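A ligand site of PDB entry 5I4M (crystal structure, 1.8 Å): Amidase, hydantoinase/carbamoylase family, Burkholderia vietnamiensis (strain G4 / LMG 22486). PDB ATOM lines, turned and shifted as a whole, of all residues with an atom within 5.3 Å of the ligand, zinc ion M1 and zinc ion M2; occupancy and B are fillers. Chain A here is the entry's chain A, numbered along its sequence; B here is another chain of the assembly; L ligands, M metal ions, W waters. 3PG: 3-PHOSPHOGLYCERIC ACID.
The guanidinium group (NH1) of Arg 309 lies within salt-bridge range of an oxygen (O2) of the ligand, at 2.8 Å.
An oxygen (O4P) of the ligand sits close to a ring nitrogen (ND1) of His 379.
An oxygen (O2) of the ligand lies within hydrogen-bond range of the side-chain amide nitrogen (NE2) of Gln 234.
ND2 of Asn 296 of chain B lies within hydrogen-bond range of O1 of the ligand, 2.8 Å away.
NE2 of His 247 of chain B lies close to O3P of the ligand.
The side-chain carboxylate (OE2) of Glu 149 lies close to an oxygen (O3) of the ligand (3.4 Å).
The backbone carbonyl oxygen (O) of Gly 378 is in hydrogen-bond range of an oxygen (O3) of the ligand (3.0 Å).
SD of Met 158 is in hydrogen-bond range of O3 of the ligand (3.3 Å).
O2 of the ligand is in hydrogen-bond range of N of Gly 378, at 2.7 Å.
NE2 of Gln 214 sits close to O3P of the ligand, at 2.9 Å.
Gln 214 touches zinc ion M2 (NE2 to ZN, 3.7 Å).
Within 4 Å of zinc ion M2: Asp 115, Glu 150, Gln 214 and His 403.
The nearest printed residue that does not touch zinc ion M2 is His 247 of chain B (4.2 Å).
Zinc ion M1 is bound by the side-chain carboxylate (OD1) of Asp 115 (2.1 Å).
Zinc ion M1 is bound by NE2 of His 104 (2.2 Å).
Water W1 binds zinc ion M1.
An oxygen (O4P) of the ligand binds zinc ion M1.
NE2 of His 211 binds zinc ion M1 (2.2 Å).
Zinc ion M1 is bound by O2P of the ligand, at 2.4 Å.
Zinc ion M1 has six donor atoms within binding distance.
Merely in contact with zinc ion M1: Gly 116 (3.7 Å) and Glu 149 (3.9 Å).
Within 4 Å of zinc ion M1: His 104, Asp 115, Gly 116, Glu 149 and His 211.
CB of Ala 157 touches O3 of the ligand (3.8 Å).
Trp 236 touches the ligand (CZ2 to O1, 3.9 Å).
Ala 377 touches the ligand.
Along chain A the residues within 4 Å of the ligand span positions 104 to 403.
The nearest printed residue that does not touch the ligand is Gly 376 (4.9 Å).
OD2 of Asp 115 sits close to NE2 of Gln 214 (3.1 Å).
The guanidinium group (NE) of Arg 309 is in salt-bridge range of the side-chain carboxylate (OD1) of Asp 307.
The backbone NH (N) of His 247 of chain B is in hydrogen-bond range of the backbone carbonyl oxygen (O) of Ser 402 (3.0 Å).
OE1 of Gln 234 is in hydrogen-bond range of NE1 of Trp 236.
The side-chain amide nitrogen (NE2) of Gln 214 lies within hydrogen-bond range of the side-chain hydroxyl (OG) of Ser 402, at 3.1 Å.
ND1 of His 403 is in hydrogen-bond range of O of Asn 296 of chain B (3.0 Å).
The backbone carbonyl oxygen of Glu 149 sits at hydrogen-bond distance from the backbone NH of Met 158, at 3.0 Å.
The side-chain amide oxygen (OE1) of Gln 234 lies close to the guanidinium group (NE) of Arg 309 (2.9 Å).
Zinc ion M2 is bound by an oxygen (O3P) of the ligand, the side-chain carboxylate (OD2) of Asp 115, the side-chain carboxylate (OE2) of Glu 150, a ring nitrogen (NE2) of His 403, an oxygen (O2P) of the ligand and the side-chain carboxylate (OE1) of Glu 150.
Water W1 lies within hydrogen-bond range of ND1 of His 379 (2.8 Å) and OE2 of Glu 149 (2.9 Å).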
ATOM      1  N   SER A 103       6.131   2.718   3.583  1.00  0.00           N
ATOM      2  CA  SER A 103       6.209   3.791   4.563  1.00  0.00           C
ATOM      3  C   SER A 103       5.948   3.169   5.927  1.00  0.00           C
ATOM      4  O   SER A 103       6.306   2.019   6.168  1.00  0.00           O
ATOM      5  CB  SER A 103       5.195   4.890   4.194  1.00  0.00           C
ATOM      6  OG  SER A 103       5.510   6.153   4.804  1.00  0.00           O
ATOM      7  N   HIS A 104       5.305   3.909   6.831  1.00  0.00           N
ATOM      8  CA  HIS A 104       5.072   3.420   8.176  1.00  0.00           C
ATOM      9  C   HIS A 104       3.597   3.447   8.512  1.00  0.00           C
ATOM     10  O   HIS A 104       2.851   4.332   8.072  1.00  0.00           O
ATOM     11  CB  HIS A 104       5.856   4.239   9.210  1.00  0.00           C
ATOM     12  CG  HIS A 104       5.568   5.706   9.158  1.00  0.00           C
ATOM     13  ND1 HIS A 104       4.724   6.325  10.057  1.00  0.00           N
ATOM     14  CD2 HIS A 104       6.026   6.680   8.343  1.00  0.00           C
ATOM     15  CE1 HIS A 104       4.666   7.618   9.785  1.00  0.00           C
ATOM     16  NE2 HIS A 104       5.451   7.859   8.753  1.00  0.00           N
ATOM     17  N   GLN A 108       2.182   9.234  15.643  1.00  0.00           N
ATOM     18  CA  GLN A 108       2.373  10.011  16.844  1.00  0.00           C
ATOM     19  C   GLN A 108       1.143   9.874  17.746  1.00  0.00           C
ATOM     20  O   GLN A 108       0.077   9.462  17.285  1.00  0.00           O
ATOM     21  CB  GLN A 108       2.581  11.477  16.479  1.00  0.00           C
ATOM     22  CG  GLN A 108       3.827  11.699  15.693  1.00  0.00           C
ATOM     23  CD  GLN A 108       5.032  11.722  16.608  1.00  0.00           C
ATOM     24  OE1 GLN A 108       4.888  11.985  17.802  1.00  0.00           O
ATOM     25  NE2 GLN A 108       6.211  11.430  16.064  1.00  0.00           N
ATOM     26  N   ASP A 115      -0.116  10.694   7.623  1.00  0.00           N
ATOM     27  CA  ASP A 115       1.336  10.568   7.785  1.00  0.00           C
ATOM     28  C   ASP A 115       1.710   9.093   7.828  1.00  0.00           C
ATOM     29  O   ASP A 115       1.159   8.327   8.634  1.00  0.00           O
ATOM     30  CB  ASP A 115       1.758  11.306   9.065  1.00  0.00           C
ATOM     31  CG  ASP A 115       3.231  11.176   9.397  1.00  0.00           C
ATOM     32  OD1 ASP A 115       4.031  10.648   8.595  1.00  0.00           O
ATOM     33  OD2 ASP A 115       3.599  11.686  10.498  1.00  0.00           O
ATOM     34  N   GLY A 116       2.584   8.680   6.914  1.00  0.00           N
ATOM     35  CA  GLY A 116       2.990   7.291   6.836  1.00  0.00           C
ATOM     36  C   GLY A 116       1.994   6.333   6.205  1.00  0.00           C
ATOM     37  O   GLY A 116       2.322   5.623   5.257  1.00  0.00           O
ATOM     38  N   GLU A 149       8.731   3.998  12.700  1.00  0.00           N
ATOM     39  CA  GLU A 149       9.389   5.058  11.960  1.00  0.00           C
ATOM     40  C   GLU A 149       9.371   6.379  12.733  1.00  0.00           C
ATOM     41  O   GLU A 149      10.303   7.171  12.588  1.00  0.00           O
ATOM     42  CB  GLU A 149       8.757   5.230  10.567  1.00  0.00           C
ATOM     43  CG  GLU A 149       9.441   6.257   9.662  1.00  0.00           C
ATOM     44  CD  GLU A 149       8.986   7.691   9.920  1.00  0.00           C
ATOM     45  OE1 GLU A 149       7.999   7.880  10.658  1.00  0.00           O
ATOM     46  OE2 GLU A 149       9.628   8.612   9.388  1.00  0.00           O
ATOM     47  N   GLU A 150       8.352   6.615  13.569  1.00  0.00           N
ATOM     48  CA  GLU A 150       8.176   7.953  14.133  1.00  0.00           C
ATOM     49  C   GLU A 150       9.253   8.281  15.166  1.00  0.00           C
ATOM     50  O   GLU A 150       9.558   9.464  15.379  1.00  0.00           O
ATOM     51  CB  GLU A 150       6.802   8.111  14.770  1.00  0.00           C
ATOM     52  CG  GLU A 150       5.632   8.221  13.785  1.00  0.00           C
ATOM     53  CD  GLU A 150       5.517   9.595  13.134  1.00  0.00           C
ATOM     54  OE1 GLU A 150       6.415  10.433  13.327  1.00  0.00           O
ATOM     55  OE2 GLU A 150       4.516   9.848  12.424  1.00  0.00           O
ATOM     56  N   ALA A 157      14.023   8.050  15.450  1.00  0.00           N
ATOM     57  CA  ALA A 157      13.204   7.721  14.293  1.00  0.00           C
ATOM     58  C   ALA A 157      13.951   6.813  13.319  1.00  0.00           C
ATOM     59  O   ALA A 157      15.173   6.716  13.333  1.00  0.00           O
ATOM     60  CB  ALA A 157      12.782   8.993  13.569  1.00  0.00           C
ATOM     61  N   MET A 158      13.170   6.146  12.466  1.00  0.00           N
ATOM     62  CA  MET A 158      13.681   5.490  11.268  1.00  0.00           C
ATOM     63  C   MET A 158      14.686   4.379  11.587  1.00  0.00           C
ATOM     64  O   MET A 158      15.551   4.060  10.763  1.00  0.00           O
ATOM     65  CB  MET A 158      14.306   6.518  10.324  1.00  0.00           C
ATOM     66  CG  MET A 158      13.314   7.579   9.832  1.00  0.00           C
ATOM     67  SD  MET A 158      14.077   9.212   9.628  1.00  0.00           S
ATOM     68  CE  MET A 158      15.432   8.827   8.526  1.00  0.00           C
ATOM     69  N   HIS A 211       4.344  10.313   0.279  1.00  0.00           N
ATOM     70  CA  HIS A 211       4.098  10.871   1.616  1.00  0.00           C
ATOM     71  C   HIS A 211       3.447  12.239   1.483  1.00  0.00           C
ATOM     72  O   HIS A 211       3.637  12.935   0.476  1.00  0.00           O
ATOM     73  CB  HIS A 211       5.417  11.006   2.383  1.00  0.00           C
ATOM     74  CG  HIS A 211       5.263  10.953   3.870  1.00  0.00           C
ATOM     75  ND1 HIS A 211       4.757  12.003   4.610  1.00  0.00           N
ATOM     76  CD2 HIS A 211       5.587   9.990   4.766  1.00  0.00           C
ATOM     77  CE1 HIS A 211       4.772  11.681   5.892  1.00  0.00           C
ATOM     78  NE2 HIS A 211       5.272  10.464   6.011  1.00  0.00           N
ATOM     79  N   GLN A 214       3.711  17.493   4.852  1.00  0.00           N
ATOM     80  CA  GLN A 214       3.822  17.858   6.258  1.00  0.00           C
ATOM     81  C   GLN A 214       4.259  19.312   6.452  1.00  0.00           C
ATOM     82  O   GLN A 214       4.666  19.701   7.546  1.00  0.00           O
ATOM     83  CB  GLN A 214       4.761  16.915   7.026  1.00  0.00           C
ATOM     84  CG  GLN A 214       4.316  15.461   6.893  1.00  0.00           C
ATOM     85  CD  GLN A 214       5.247  14.523   7.617  1.00  0.00           C
ATOM     86  OE1 GLN A 214       6.375  14.313   7.160  1.00  0.00           O
ATOM     87  NE2 GLN A 214       4.791  13.955   8.727  1.00  0.00           N
ATOM     88  N   GLN A 234      19.170  15.869  10.245  1.00  0.00           N
ATOM     89  CA  GLN A 234      18.653  16.010  11.600  1.00  0.00           C
ATOM     90  C   GLN A 234      19.703  15.603  12.623  1.00  0.00           C
ATOM     91  O   GLN A 234      20.546  14.742  12.364  1.00  0.00           O
ATOM     92  CB  GLN A 234      17.410  15.153  11.827  1.00  0.00           C
ATOM     93  CG  GLN A 234      16.303  15.324  10.803  1.00  0.00           C
ATOM     94  CD  GLN A 234      14.969  14.810  11.319  1.00  0.00           C
ATOM     95  OE1 GLN A 234      14.549  15.175  12.413  1.00  0.00           O
ATOM     96  NE2 GLN A 234      14.315  13.952  10.549  1.00  0.00           N
ATOM     97  N   TRP A 236      19.217  14.728  16.852  1.00  0.00           N
ATOM     98  CA  TRP A 236      18.366  14.651  18.033  1.00  0.00           C
ATOM     99  C   TRP A 236      19.223  14.408  19.273  1.00  0.00           C
ATOM    100  O   TRP A 236      20.229  13.704  19.223  1.00  0.00           O
ATOM    101  CB  TRP A 236      17.341  13.516  17.940  1.00  0.00           C
ATOM    102  CG  TRP A 236      16.305  13.648  16.861  1.00  0.00           C
ATOM    103  CD1 TRP A 236      16.282  14.531  15.824  1.00  0.00           C
ATOM    104  CD2 TRP A 236      15.128  12.843  16.742  1.00  0.00           C
ATOM    105  NE1 TRP A 236      15.147  14.326  15.055  1.00  0.00           N
ATOM    106  CE2 TRP A 236      14.436  13.288  15.597  1.00  0.00           C
ATOM    107  CE3 TRP A 236      14.597  11.777  17.488  1.00  0.00           C
ATOM    108  CZ2 TRP A 236      13.225  12.713  15.178  1.00  0.00           C
ATOM    109  CZ3 TRP A 236      13.405  11.213  17.090  1.00  0.00           C
ATOM    110  CH2 TRP A 236      12.722  11.678  15.941  1.00  0.00           C
ATOM    111  N   ASP A 307      15.550  18.684  19.157  1.00  0.00           N
ATOM    112  CA  ASP A 307      15.336  18.287  17.767  1.00  0.00           C
ATOM    113  C   ASP A 307      15.869  19.428  16.909  1.00  0.00           C
ATOM    114  O   ASP A 307      15.342  20.544  16.977  1.00  0.00           O
ATOM    115  CB  ASP A 307      13.849  18.037  17.516  1.00  0.00           C
ATOM    116  CG  ASP A 307      13.527  17.605  16.080  1.00  0.00           C
ATOM    117  OD1 ASP A 307      13.909  18.286  15.120  1.00  0.00           O
ATOM    118  OD2 ASP A 307      12.843  16.566  15.952  1.00  0.00           O
ATOM    119  N   ARG A 309      17.185  20.481  12.870  1.00  0.00           N
ATOM    120  CA  ARG A 309      17.202  20.079  11.458  1.00  0.00           C
ATOM    121  C   ARG A 309      17.685  21.246  10.608  1.00  0.00           C
ATOM    122  O   ARG A 309      17.408  22.412  10.912  1.00  0.00           O
ATOM    123  CB  ARG A 309      15.804  19.660  10.979  1.00  0.00           C
ATOM    124  CG  ARG A 309      15.044  18.852  12.018  1.00  0.00           C
ATOM    125  CD  ARG A 309      13.699  18.384  11.496  1.00  0.00           C
ATOM    126  NE  ARG A 309      13.010  17.665  12.563  1.00  0.00           N
ATOM    127  CZ  ARG A 309      12.124  16.708  12.360  1.00  0.00           C
ATOM    128  NH1 ARG A 309      11.793  16.353  11.122  1.00  0.00           N
ATOM    129  NH2 ARG A 309      11.591  16.067  13.396  1.00  0.00           N
ATOM    130  N   TYR A 346      21.721  12.217  10.966  1.00  0.00           N
ATOM    131  CA  TYR A 346      22.050  11.877   9.586  1.00  0.00           C
ATOM    132  C   TYR A 346      22.182  13.153   8.771  1.00  0.00           C
ATOM    133  O   TYR A 346      21.478  14.143   9.026  1.00  0.00           O
ATOM    134  CB  TYR A 346      21.020  10.926   8.949  1.00  0.00           C
ATOM    135  CG  TYR A 346      19.616  11.464   8.785  1.00  0.00           C
ATOM    136  CD1 TYR A 346      19.240  12.125   7.615  1.00  0.00           C
ATOM    137  CD2 TYR A 346      18.645  11.258   9.766  1.00  0.00           C
ATOM    138  CE1 TYR A 346      17.943  12.601   7.436  1.00  0.00           C
ATOM    139  CE2 TYR A 346      17.353  11.730   9.600  1.00  0.00           C
ATOM    140  CZ  TYR A 346      17.010  12.402   8.452  1.00  0.00           C
ATOM    141  OH  TYR A 346      15.723  12.856   8.301  1.00  0.00           O
ATOM    142  N   GLY A 376      11.227  18.097   4.752  1.00  0.00           N
ATOM    143  CA  GLY A 376      11.594  18.657   6.037  1.00  0.00           C
ATOM    144  C   GLY A 376      11.562  17.615   7.128  1.00  0.00           C
ATOM    145  O   GLY A 376      12.190  17.771   8.180  1.00  0.00           O
ATOM    146  N   ALA A 377      10.812  16.534   6.898  1.00  0.00           N
ATOM    147  CA  ALA A 377      10.787  15.406   7.813  1.00  0.00           C
ATOM    148  C   ALA A 377      11.750  14.329   7.342  1.00  0.00           C
ATOM    149  O   ALA A 377      12.222  14.337   6.205  1.00  0.00           O
ATOM    150  CB  ALA A 377       9.373  14.832   7.930  1.00  0.00           C
ATOM    151  N   GLY A 378      12.038  13.405   8.245  1.00  0.00           N
ATOM    152  CA  GLY A 378      12.734  12.186   7.880  1.00  0.00           C
ATOM    153  C   GLY A 378      11.747  11.120   7.442  1.00  0.00           C
ATOM    154  O   GLY A 378      10.587  11.109   7.877  1.00  0.00           O
ATOM    155  N   HIS A 379      12.203  10.233   6.574  1.00  0.00           N
ATOM    156  CA  HIS A 379      11.406   9.129   6.085  1.00  0.00           C
ATOM    157  C   HIS A 379      12.295   7.917   5.949  1.00  0.00           C
ATOM    158  O   HIS A 379      13.513   8.033   5.817  1.00  0.00           O
ATOM    159  CB  HIS A 379      10.758   9.460   4.746  1.00  0.00           C
ATOM    160  CG  HIS A 379      10.044  10.763   4.756  1.00  0.00           C
ATOM    161  ND1 HIS A 379       8.782  10.906   5.296  1.00  0.00           N
ATOM    162  CD2 HIS A 379      10.417  11.995   4.334  1.00  0.00           C
ATOM    163  CE1 HIS A 379       8.410  12.163   5.193  1.00  0.00           C
ATOM    164  NE2 HIS A 379       9.372  12.843   4.613  1.00  0.00           N
ATOM    165  N   SER A 402       0.927  18.685  10.229  1.00  0.00           N
ATOM    166  CA  SER A 402       1.097  17.265  10.483  1.00  0.00           C
ATOM    167  C   SER A 402       1.494  17.123  11.943  1.00  0.00           C
ATOM    168  O   SER A 402       1.822  18.107  12.612  1.00  0.00           O
ATOM    169  CB  SER A 402       2.132  16.640   9.546  1.00  0.00           C
ATOM    170  OG  SER A 402       2.218  15.248   9.742  1.00  0.00           O
ATOM    171  N   HIS A 403       1.432  15.899  12.442  1.00  0.00           N
ATOM    172  CA  HIS A 403       1.629  15.599  13.865  1.00  0.00           C
ATOM    173  C   HIS A 403       0.599  16.315  14.728  1.00  0.00           C
ATOM    174  O   HIS A 403       0.853  16.629  15.894  1.00  0.00           O
ATOM    175  CB  HIS A 403       3.066  15.895  14.296  1.00  0.00           C
ATOM    176  CG  HIS A 403       4.041  14.860  13.795  1.00  0.00           C
ATOM    177  ND1 HIS A 403       5.344  14.767  14.243  1.00  0.00           N
ATOM    178  CD2 HIS A 403       3.871  13.868  12.888  1.00  0.00           C
ATOM    179  CE1 HIS A 403       5.934  13.759  13.637  1.00  0.00           C
ATOM    180  NE2 HIS A 403       5.067  13.192  12.813  1.00  0.00           N
ATOM    181  N   HIS B 247       4.292  19.498  13.520  1.00  0.00           N
ATOM    182  CA  HIS B 247       5.520  18.750  13.280  1.00  0.00           C
ATOM    183  C   HIS B 247       6.743  19.569  13.713  1.00  0.00           C
ATOM    184  O   HIS B 247       6.857  20.758  13.415  1.00  0.00           O
ATOM    185  CB  HIS B 247       5.648  18.398  11.795  1.00  0.00           C
ATOM    186  CG  HIS B 247       6.471  17.187  11.558  1.00  0.00           C
ATOM    187  ND1 HIS B 247       7.817  17.131  11.836  1.00  0.00           N
ATOM    188  CD2 HIS B 247       6.137  15.949  11.105  1.00  0.00           C
ATOM    189  CE1 HIS B 247       8.283  15.924  11.554  1.00  0.00           C
ATOM    190  NE2 HIS B 247       7.278  15.191  11.106  1.00  0.00           N
ATOM    191  N   ASN B 296       9.339  14.749  18.631  1.00  0.00           N
ATOM    192  CA  ASN B 296       9.214  15.402  17.337  1.00  0.00           C
ATOM    193  C   ASN B 296       7.819  15.996  17.109  1.00  0.00           C
ATOM    194  O   ASN B 296       7.359  16.095  15.972  1.00  0.00           O
ATOM    195  CB  ASN B 296       9.648  14.475  16.176  1.00  0.00           C
ATOM    196  CG  ASN B 296       9.019  13.079  16.214  1.00  0.00           C
ATOM    197  OD1 ASN B 296       8.454  12.635  17.208  1.00  0.00           O
ATOM    198  ND2 ASN B 296       9.169  12.353  15.093  1.00  0.00           N
HETATM  199  C1  3PG L   1      10.658  13.084  11.765  1.00  0.00           C
HETATM  200  O1  3PG L   1      10.305  13.639  12.821  1.00  0.00           O
HETATM  201  O2  3PG L   1      10.997  13.732  10.746  1.00  0.00           O
HETATM  202  C2  3PG L   1      10.684  11.582  11.731  1.00  0.00           C
HETATM  203  O3  3PG L   1      11.546  11.121  10.672  1.00  0.00           O
HETATM  204  C3  3PG L   1       9.277  11.094  11.476  1.00  0.00           C
HETATM  205  O1P 3PG L   1       8.861  11.514  10.173  1.00  0.00           O
HETATM  206  P   3PG L   1       7.269  11.471   9.786  1.00  0.00           P
HETATM  207  O2P 3PG L   1       6.750  10.138  10.268  1.00  0.00           O
HETATM  208  O3P 3PG L   1       6.676  12.636  10.560  1.00  0.00           O
HETATM  209  O4P 3PG L   1       7.274  11.608   8.250  1.00  0.00           O
HETATM  210 ZN    ZN M   1       5.936   9.867   8.071  1.00  0.00          ZN
HETATM  211 ZN    ZN M   2       5.333  11.507  11.515  1.00  0.00          ZN
HETATM  212  O   HOH W   1       7.753   9.050   7.161  1.00  0.00           O
